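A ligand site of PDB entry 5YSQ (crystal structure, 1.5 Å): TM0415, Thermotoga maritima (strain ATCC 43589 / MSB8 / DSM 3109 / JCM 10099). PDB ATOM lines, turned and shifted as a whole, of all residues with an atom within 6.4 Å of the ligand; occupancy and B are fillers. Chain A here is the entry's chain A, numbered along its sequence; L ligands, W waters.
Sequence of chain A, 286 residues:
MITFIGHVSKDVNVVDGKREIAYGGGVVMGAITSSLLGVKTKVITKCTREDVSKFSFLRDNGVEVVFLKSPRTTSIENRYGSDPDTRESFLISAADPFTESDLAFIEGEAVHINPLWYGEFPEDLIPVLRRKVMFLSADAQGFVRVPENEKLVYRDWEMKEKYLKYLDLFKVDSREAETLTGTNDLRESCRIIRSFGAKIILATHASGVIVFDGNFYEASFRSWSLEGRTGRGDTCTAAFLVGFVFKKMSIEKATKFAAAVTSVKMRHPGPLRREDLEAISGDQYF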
ATOM      1  N   SER A   9     -15.332 -21.624 -29.731  1.00  0.00           N
ATOM      2  CA  SER A   9     -15.061 -22.875 -30.419  1.00  0.00           C
ATOM      3  C   SER A   9     -15.827 -22.987 -31.702  1.00  0.00           C
ATOM      4  O   SER A   9     -17.024 -22.668 -31.764  1.00  0.00           O
ATOM      5  CB  SER A   9     -15.464 -24.065 -29.543  1.00  0.00           C
ATOM      6  OG  SER A   9     -15.238 -25.308 -30.195  1.00  0.00           O
ATOM      7  N   LYS A  10     -15.142 -23.518 -32.714  1.00  0.00           N
ATOM      8  CA  LYS A  10     -15.836 -24.095 -33.880  1.00  0.00           C
ATOM      9  C   LYS A  10     -16.221 -25.523 -33.493  1.00  0.00           C
ATOM     10  O   LYS A  10     -15.365 -26.385 -33.465  1.00  0.00           O
ATOM     11  CB  LYS A  10     -14.929 -24.130 -35.098  1.00  0.00           C
ATOM     12  CG  LYS A  10     -15.566 -24.724 -36.332  1.00  0.00           C
ATOM     13  CD  LYS A  10     -14.563 -24.992 -37.449  1.00  0.00           C
ATOM     14  CE  LYS A  10     -15.180 -25.710 -38.613  1.00  0.00           C
ATOM     15  NZ  LYS A  10     -14.227 -25.858 -39.715  1.00  0.00           N
ATOM     16  N   ASP A  11     -17.500 -25.733 -33.203  1.00  0.00           N
ATOM     17  CA  ASP A  11     -18.023 -27.044 -32.829  1.00  0.00           C
ATOM     18  C   ASP A  11     -18.355 -27.815 -34.091  1.00  0.00           C
ATOM     19  O   ASP A  11     -19.071 -27.323 -34.960  1.00  0.00           O
ATOM     20  CB  ASP A  11     -19.235 -26.889 -31.953  1.00  0.00           C
ATOM     21  CG  ASP A  11     -18.912 -26.352 -30.548  1.00  0.00           C
ATOM     22  OD1 ASP A  11     -17.737 -26.397 -30.103  1.00  0.00           O
ATOM     23  OD2 ASP A  11     -19.885 -25.914 -29.876  1.00  0.00           O
ATOM     24  N   VAL A  12     -17.857 -29.055 -34.144  1.00  0.00           N
ATOM     25  CA  VAL A  12     -18.176 -29.982 -35.229  1.00  0.00           C
ATOM     26  C   VAL A  12     -19.080 -31.014 -34.628  1.00  0.00           C
ATOM     27  O   VAL A  12     -18.632 -31.918 -33.930  1.00  0.00           O
ATOM     28  CB  VAL A  12     -16.909 -30.635 -35.828  1.00  0.00           C
ATOM     29  CG1 VAL A  12     -17.288 -31.567 -36.974  1.00  0.00           C
ATOM     30  CG2 VAL A  12     -15.935 -29.569 -36.282  1.00  0.00           C
ATOM     31  N   ASN A  13     -20.377 -30.827 -34.850  1.00  0.00           N
ATOM     32  CA  ASN A  13     -21.366 -31.697 -34.234  1.00  0.00           C
ATOM     33  C   ASN A  13     -21.727 -32.779 -35.195  1.00  0.00           C
ATOM     34  O   ASN A  13     -22.170 -32.483 -36.309  1.00  0.00           O
ATOM     35  CB  ASN A  13     -22.578 -30.873 -33.795  1.00  0.00           C
ATOM     36  CG  ASN A  13     -22.249 -29.887 -32.695  1.00  0.00           C
ATOM     37  OD1 ASN A  13     -21.457 -30.177 -31.788  1.00  0.00           O
ATOM     38  ND2 ASN A  13     -22.741 -28.634 -32.808  1.00  0.00           N
ATOM     39  N   GLY A  24     -19.662 -21.655 -31.178  1.00  0.00           N
ATOM     40  CA  GLY A  24     -20.096 -21.604 -29.808  1.00  0.00           C
ATOM     41  C   GLY A  24     -18.923 -21.505 -28.845  1.00  0.00           C
ATOM     42  O   GLY A  24     -17.993 -20.683 -29.079  1.00  0.00           O
ATOM     43  N   GLY A  25     -19.090 -22.323 -27.801  1.00  0.00           N
ATOM     44  CA  GLY A  25     -18.240 -22.337 -26.626  1.00  0.00           C
ATOM     45  C   GLY A  25     -18.967 -21.876 -25.372  1.00  0.00           C
ATOM     46  O   GLY A  25     -20.084 -21.360 -25.425  1.00  0.00           O
ATOM     47  N   GLY A  26     -18.377 -22.149 -24.211  1.00  0.00           N
ATOM     48  CA  GLY A  26     -19.055 -21.886 -22.945  1.00  0.00           C
ATOM     49  C   GLY A  26     -19.245 -20.376 -22.785  1.00  0.00           C
ATOM     50  O   GLY A  26     -20.281 -19.953 -22.267  1.00  0.00           O
ATOM     51  N   MET A  29     -22.396 -19.076 -24.625  1.00  0.00           N
ATOM     52  CA  MET A  29     -23.659 -19.389 -23.998  1.00  0.00           C
ATOM     53  C   MET A  29     -23.864 -18.546 -22.700  1.00  0.00           C
ATOM     54  O   MET A  29     -24.952 -18.016 -22.484  1.00  0.00           O
ATOM     55  CB  MET A  29     -23.723 -20.893 -23.695  1.00  0.00           C
ATOM     56  CG  MET A  29     -23.827 -21.799 -24.897  1.00  0.00           C
ATOM     57  SD  MET A  29     -25.519 -21.788 -25.493  1.00  0.00           S
ATOM     58  CE  MET A  29     -25.449 -22.993 -26.827  1.00  0.00           C
ATOM     59  N   ILE A  76     -13.826 -28.283 -31.379  1.00  0.00           N
ATOM     60  CA  ILE A  76     -14.174 -29.515 -30.637  1.00  0.00           C
ATOM     61  C   ILE A  76     -15.170 -30.268 -31.503  1.00  0.00           C
ATOM     62  O   ILE A  76     -16.161 -29.704 -31.894  1.00  0.00           O
ATOM     63  CB  ILE A  76     -14.737 -29.148 -29.287  1.00  0.00           C
ATOM     64  CG1 ILE A  76     -13.600 -28.506 -28.458  1.00  0.00           C
ATOM     65  CG2 ILE A  76     -15.267 -30.359 -28.532  1.00  0.00           C
ATOM     66  CD1 ILE A  76     -14.036 -27.976 -27.175  1.00  0.00           C
ATOM     67  N   GLU A  77     -14.938 -31.562 -31.661  1.00  0.00           N
ATOM     68  CA  GLU A  77     -15.913 -32.443 -32.336  1.00  0.00           C
ATOM     69  C   GLU A  77     -16.741 -33.118 -31.251  1.00  0.00           C
ATOM     70  O   GLU A  77     -16.208 -33.698 -30.331  1.00  0.00           O
ATOM     71  CB  GLU A  77     -15.231 -33.488 -33.199  1.00  0.00           C
ATOM     72  CG  GLU A  77     -16.227 -34.430 -33.879  1.00  0.00           C
ATOM     73  CD  GLU A  77     -15.535 -35.433 -34.742  1.00  0.00           C
ATOM     74  OE1 GLU A  77     -14.673 -35.038 -35.522  1.00  0.00           O
ATOM     75  OE2 GLU A  77     -15.860 -36.617 -34.613  1.00  0.00           O
ATOM     76  N   ASN A  78     -18.065 -33.055 -31.358  1.00  0.00           N
ATOM     77  CA  ASN A  78     -18.981 -33.702 -30.436  1.00  0.00           C
ATOM     78  C   ASN A  78     -19.713 -34.764 -31.199  1.00  0.00           C
ATOM     79  O   ASN A  78     -20.396 -34.452 -32.182  1.00  0.00           O
ATOM     80  CB  ASN A  78     -19.954 -32.676 -29.888  1.00  0.00           C
ATOM     81  CG  ASN A  78     -19.256 -31.559 -29.152  1.00  0.00           C
ATOM     82  OD1 ASN A  78     -18.542 -31.790 -28.156  1.00  0.00           O
ATOM     83  ND2 ASN A  78     -19.425 -30.342 -29.656  1.00  0.00           N
ATOM     84  N   TYR A  80     -22.498 -37.900 -31.097  1.00  0.00           N
ATOM     85  CA  TYR A  80     -23.734 -38.336 -30.423  1.00  0.00           C
ATOM     86  C   TYR A  80     -24.143 -39.565 -31.145  1.00  0.00           C
ATOM     87  O   TYR A  80     -24.229 -39.507 -32.372  1.00  0.00           O
ATOM     88  CB  TYR A  80     -24.849 -37.287 -30.568  1.00  0.00           C
ATOM     89  CG  TYR A  80     -24.479 -35.927 -30.027  1.00  0.00           C
ATOM     90  CD1 TYR A  80     -24.440 -35.693 -28.642  1.00  0.00           C
ATOM     91  CD2 TYR A  80     -24.127 -34.862 -30.893  1.00  0.00           C
ATOM     92  CE1 TYR A  80     -24.078 -34.450 -28.127  1.00  0.00           C
ATOM     93  CE2 TYR A  80     -23.749 -33.611 -30.380  1.00  0.00           C
ATOM     94  CZ  TYR A  80     -23.727 -33.408 -29.001  1.00  0.00           C
ATOM     95  OH  TYR A  80     -23.364 -32.165 -28.486  1.00  0.00           O
ATOM     96  N   SER A  89     -16.407 -36.170 -26.902  1.00  0.00           N
ATOM     97  CA  SER A  89     -15.858 -34.994 -27.532  1.00  0.00           C
ATOM     98  C   SER A  89     -14.359 -35.120 -27.754  1.00  0.00           C
ATOM     99  O   SER A  89     -13.689 -35.898 -27.063  1.00  0.00           O
ATOM    100  CB  SER A  89     -16.156 -33.776 -26.674  1.00  0.00           C
ATOM    101  OG  SER A  89     -17.531 -33.666 -26.476  1.00  0.00           O
ATOM    102  N   PRO A 115     -13.531 -22.534 -19.171  1.00  0.00           N
ATOM    103  CA  PRO A 115     -12.706 -23.198 -20.172  1.00  0.00           C
ATOM    104  C   PRO A 115     -13.295 -24.434 -20.754  1.00  0.00           C
ATOM    105  O   PRO A 115     -14.154 -25.099 -20.123  1.00  0.00           O
ATOM    106  CB  PRO A 115     -11.414 -23.531 -19.395  1.00  0.00           C
ATOM    107  CG  PRO A 115     -11.625 -23.026 -17.952  1.00  0.00           C
ATOM    108  CD  PRO A 115     -13.092 -22.976 -17.832  1.00  0.00           C
ATOM    109  N   LEU A 116     -12.813 -24.831 -21.917  1.00  0.00           N
ATOM    110  CA  LEU A 116     -13.327 -26.007 -22.617  1.00  0.00           C
ATOM    111  C   LEU A 116     -12.481 -27.249 -22.361  1.00  0.00           C
ATOM    112  O   LEU A 116     -12.929 -28.379 -22.574  1.00  0.00           O
ATOM    113  CB  LEU A 116     -13.404 -25.737 -24.102  1.00  0.00           C
ATOM    114  CG  LEU A 116     -14.475 -24.745 -24.495  1.00  0.00           C
ATOM    115  CD1 LEU A 116     -14.352 -24.320 -25.952  1.00  0.00           C
ATOM    116  CD2 LEU A 116     -15.844 -25.396 -24.274  1.00  0.00           C
ATOM    117  N   GLN A 141     -15.426 -28.149 -15.984  1.00  0.00           N
ATOM    118  CA  GLN A 141     -15.078 -28.684 -17.295  1.00  0.00           C
ATOM    119  C   GLN A 141     -13.617 -28.331 -17.668  1.00  0.00           C
ATOM    120  O   GLN A 141     -12.905 -29.150 -18.275  1.00  0.00           O
ATOM    121  CB  GLN A 141     -15.998 -28.114 -18.353  1.00  0.00           C
ATOM    122  CG  GLN A 141     -15.712 -28.613 -19.716  1.00  0.00           C
ATOM    123  CD  GLN A 141     -16.698 -28.047 -20.697  1.00  0.00           C
ATOM    124  OE1 GLN A 141     -17.629 -28.741 -21.120  1.00  0.00           O
ATOM    125  NE2 GLN A 141     -16.605 -26.729 -20.957  1.00  0.00           N
ATOM    126  N   ARG A 145     -11.726 -32.074 -17.953  1.00  0.00           N
ATOM    127  CA  ARG A 145     -11.820 -32.555 -19.274  1.00  0.00           C
ATOM    128  C   ARG A 145     -10.461 -32.397 -19.991  1.00  0.00           C
ATOM    129  O   ARG A 145     -10.110 -31.284 -20.371  1.00  0.00           O
ATOM    130  CB  ARG A 145     -12.991 -31.850 -19.942  1.00  0.00           C
ATOM    131  CG  ARG A 145     -13.388 -32.572 -21.190  1.00  0.00           C
ATOM    132  CD  ARG A 145     -14.721 -32.162 -21.755  1.00  0.00           C
ATOM    133  NE  ARG A 145     -14.565 -30.922 -22.512  1.00  0.00           N
ATOM    134  CZ  ARG A 145     -15.470 -30.470 -23.370  1.00  0.00           C
ATOM    135  NH1 ARG A 145     -16.600 -31.127 -23.632  1.00  0.00           N
ATOM    136  NH2 ARG A 145     -15.247 -29.319 -23.970  1.00  0.00           N
ATOM    137  N   LEU A 152     -11.365 -36.048 -25.379  1.00  0.00           N
ATOM    138  CA  LEU A 152     -11.488 -35.302 -24.107  1.00  0.00           C
ATOM    139  C   LEU A 152     -11.966 -36.305 -23.065  1.00  0.00           C
ATOM    140  O   LEU A 152     -13.131 -36.728 -23.080  1.00  0.00           O
ATOM    141  CB  LEU A 152     -12.415 -34.095 -24.279  1.00  0.00           C
ATOM    142  CG  LEU A 152     -11.758 -32.973 -25.082  1.00  0.00           C
ATOM    143  CD1 LEU A 152     -12.827 -32.079 -25.674  1.00  0.00           C
ATOM    144  CD2 LEU A 152     -10.717 -32.212 -24.238  1.00  0.00           C
ATOM    145  N   ARG A 229     -29.859 -28.893 -25.675  1.00  0.00           N
ATOM    146  CA  ARG A 229     -29.233 -29.257 -24.396  1.00  0.00           C
ATOM    147  C   ARG A 229     -27.788 -28.691 -24.260  1.00  0.00           C
ATOM    148  O   ARG A 229     -27.364 -28.353 -23.150  1.00  0.00           O
ATOM    149  CB  ARG A 229     -29.348 -30.796 -24.192  1.00  0.00           C
ATOM    150  CG  ARG A 229     -28.597 -31.313 -22.979  1.00  0.00           C
ATOM    151  CD  ARG A 229     -27.216 -31.807 -23.361  1.00  0.00           C
ATOM    152  NE  ARG A 229     -26.469 -32.292 -22.189  1.00  0.00           N
ATOM    153  CZ  ARG A 229     -25.842 -31.512 -21.297  1.00  0.00           C
ATOM    154  NH1 ARG A 229     -25.852 -30.191 -21.401  1.00  0.00           N
ATOM    155  NH2 ARG A 229     -25.187 -32.086 -20.298  1.00  0.00           N
ATOM    156  N   THR A 230     -27.051 -28.588 -25.369  1.00  0.00           N
ATOM    157  CA  THR A 230     -25.717 -28.003 -25.327  1.00  0.00           C
ATOM    158  C   THR A 230     -25.817 -26.569 -24.813  1.00  0.00           C
ATOM    159  O   THR A 230     -26.701 -25.844 -25.194  1.00  0.00           O
ATOM    160  CB  THR A 230     -25.016 -27.997 -26.700  1.00  0.00           C
ATOM    161  OG1 THR A 230     -24.762 -29.365 -27.017  1.00  0.00           O
ATOM    162  CG2 THR A 230     -23.710 -27.240 -26.660  1.00  0.00           C
ATOM    163  N   GLY A 231     -24.938 -26.198 -23.899  1.00  0.00           N
ATOM    164  CA  GLY A 231     -24.969 -24.896 -23.281  1.00  0.00           C
ATOM    165  C   GLY A 231     -25.876 -24.743 -22.079  1.00  0.00           C
ATOM    166  O   GLY A 231     -25.996 -23.660 -21.519  1.00  0.00           O
ATOM    167  N   ARG A 232     -26.533 -25.836 -21.677  1.00  0.00           N
ATOM    168  CA  ARG A 232     -27.357 -25.906 -20.465  1.00  0.00           C
ATOM    169  C   ARG A 232     -26.626 -25.307 -19.283  1.00  0.00           C
ATOM    170  O   ARG A 232     -27.148 -24.475 -18.560  1.00  0.00           O
ATOM    171  CB  ARG A 232     -27.695 -27.369 -20.152  1.00  0.00           C
ATOM    172  CG  ARG A 232     -28.546 -27.630 -18.929  1.00  0.00           C
ATOM    173  CD  ARG A 232     -28.743 -29.093 -18.650  1.00  0.00           C
ATOM    174  NE  ARG A 232     -27.551 -29.737 -18.141  1.00  0.00           N
ATOM    175  CZ  ARG A 232     -27.425 -31.039 -17.906  1.00  0.00           C
ATOM    176  NH1 ARG A 232     -28.411 -31.857 -18.180  1.00  0.00           N
ATOM    177  NH2 ARG A 232     -26.252 -31.508 -17.423  1.00  0.00           N
ATOM    178  N   ASP A 234     -23.720 -23.682 -18.943  1.00  0.00           N
ATOM    179  CA  ASP A 234     -23.211 -22.310 -19.031  1.00  0.00           C
ATOM    180  C   ASP A 234     -24.339 -21.282 -18.908  1.00  0.00           C
ATOM    181  O   ASP A 234     -24.227 -20.231 -18.248  1.00  0.00           O
ATOM    182  CB  ASP A 234     -22.512 -22.087 -20.344  1.00  0.00           C
ATOM    183  CG  ASP A 234     -21.255 -22.807 -20.440  1.00  0.00           C
ATOM    184  OD1 ASP A 234     -20.378 -22.426 -19.670  1.00  0.00           O
ATOM    185  OD2 ASP A 234     -21.122 -23.697 -21.304  1.00  0.00           O
HETATM  186  C1  LIG L   1     -20.278 -27.543 -24.538  1.00  0.00           C
HETATM  187  C2  LIG L   1     -19.208 -28.638 -24.503  1.00  0.00           C
HETATM  188  C3  LIG L   1     -18.875 -29.037 -25.942  1.00  0.00           C
HETATM  189  C4  LIG L   1     -18.313 -27.820 -26.724  1.00  0.00           C
HETATM  190  C5  LIG L   1     -19.313 -26.687 -26.734  1.00  0.00           C
HETATM  191  C6  LIG L   1     -19.741 -26.343 -25.288  1.00  0.00           C
HETATM  192  O1  LIG L   1     -20.598 -27.171 -23.190  1.00  0.00           O
HETATM  193  O2  LIG L   1     -18.024 -28.197 -23.887  1.00  0.00           O
HETATM  194  O3  LIG L   1     -18.013 -30.141 -25.955  1.00  0.00           O
HETATM  195  O4  LIG L   1     -18.042 -28.246 -28.066  1.00  0.00           O
HETATM  196  O5  LIG L   1     -18.700 -25.510 -27.333  1.00  0.00           O
HETATM  197  O6  LIG L   1     -20.702 -25.244 -25.415  1.00  0.00           O
HETATM  198  O   HOH W   1     -23.119 -28.029 -22.616  1.00  0.00           O
HETATM  199  O   HOH W   2     -19.019 -25.275 -21.925  1.00  0.00           O
HETATM  200  O   HOH W   3     -21.389 -24.339 -28.163  1.00  0.00           O
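The side-chain amide oxygen (OD1) of Asn 78 sits at hydrogen-bond distance from the side-chain hydroxyl (OG) of Ser 89.
The backbone carbonyl oxygen (O) of Val 12 lies within hydrogen-bond range of the backbone NH (N) of Asn 78.
The side-chain hydroxyl of Ser 9 lies within hydrogen-bond range of the side-chain carboxylate of Asp 11, 2.7 Å away.
The side-chain hydroxyl of Tyr 80 is in hydrogen-bond range of the side-chain hydroxyl of Thr 230, at 3.5 Å.
The backbone NH (N) of Ile 76 lies within hydrogen-bond range of the backbone carbonyl oxygen (O) of Lys 10, at 3.2 Å.
O of Ser 89 is in hydrogen-bond range of N of Leu 152.
O of Ile 76 lies within hydrogen-bond range of N of Val 12.
O of Pro 115 lies within hydrogen-bond range of NE2 of Gln 141 (3.1 Å).
OE1 of Gln 141 is in hydrogen-bond range of O2 of the ligand, at 2.8 Å.
An oxygen (O4) of the ligand is in hydrogen-bond range of the side-chain carboxylate (OD1) of Asp 11.
The guanidinium group (NH1) of Arg 145 is in hydrogen-bond range of an oxygen (O3) of the ligand (2.9 Å).
OD1 of Asn 78 is in hydrogen-bond range of O3 of the ligand (2.8 Å).
O5 of the ligand lies within hydrogen-bond range of N of Gly 25, 3.2 Å away.
CG2 of Ile 76 touches O4 of the ligand, at 3.5 Å.
Ser 89 touches the ligand (OG to O3, 3.6 Å).
Leu 116 touches the ligand.
Thr 230 touches the ligand (CG2 to O6, 3.8 Å).
OD2 of Asp 234 touches O1 of the ligand (3.99 Å).
Hydrophobic or aromatic side chains that line the ligand: Ile 76 and Leu 116.
Within 4 Å of the ligand: Asp 11, Gly 25, Ile 76, Asn 78, Ser 89, Leu 116, Gln 141, Arg 145, Thr 230 and Asp 234.
Water W1 lies within hydrogen-bond range of an oxygen (O1) of the ligand and the backbone NH (N) of Gly 231.
Water W2 lies within hydrogen-bond range of the side-chain carboxylate of Asp 234, an oxygen (O1) of the ligand and the side-chain amide nitrogen of Gln 141.
Water W3 lies within hydrogen-bond range of OD2 of Asp 11 (2.8 Å), O6 of the ligand (3.0 Å) and N of Gly 25 (3.1 Å).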
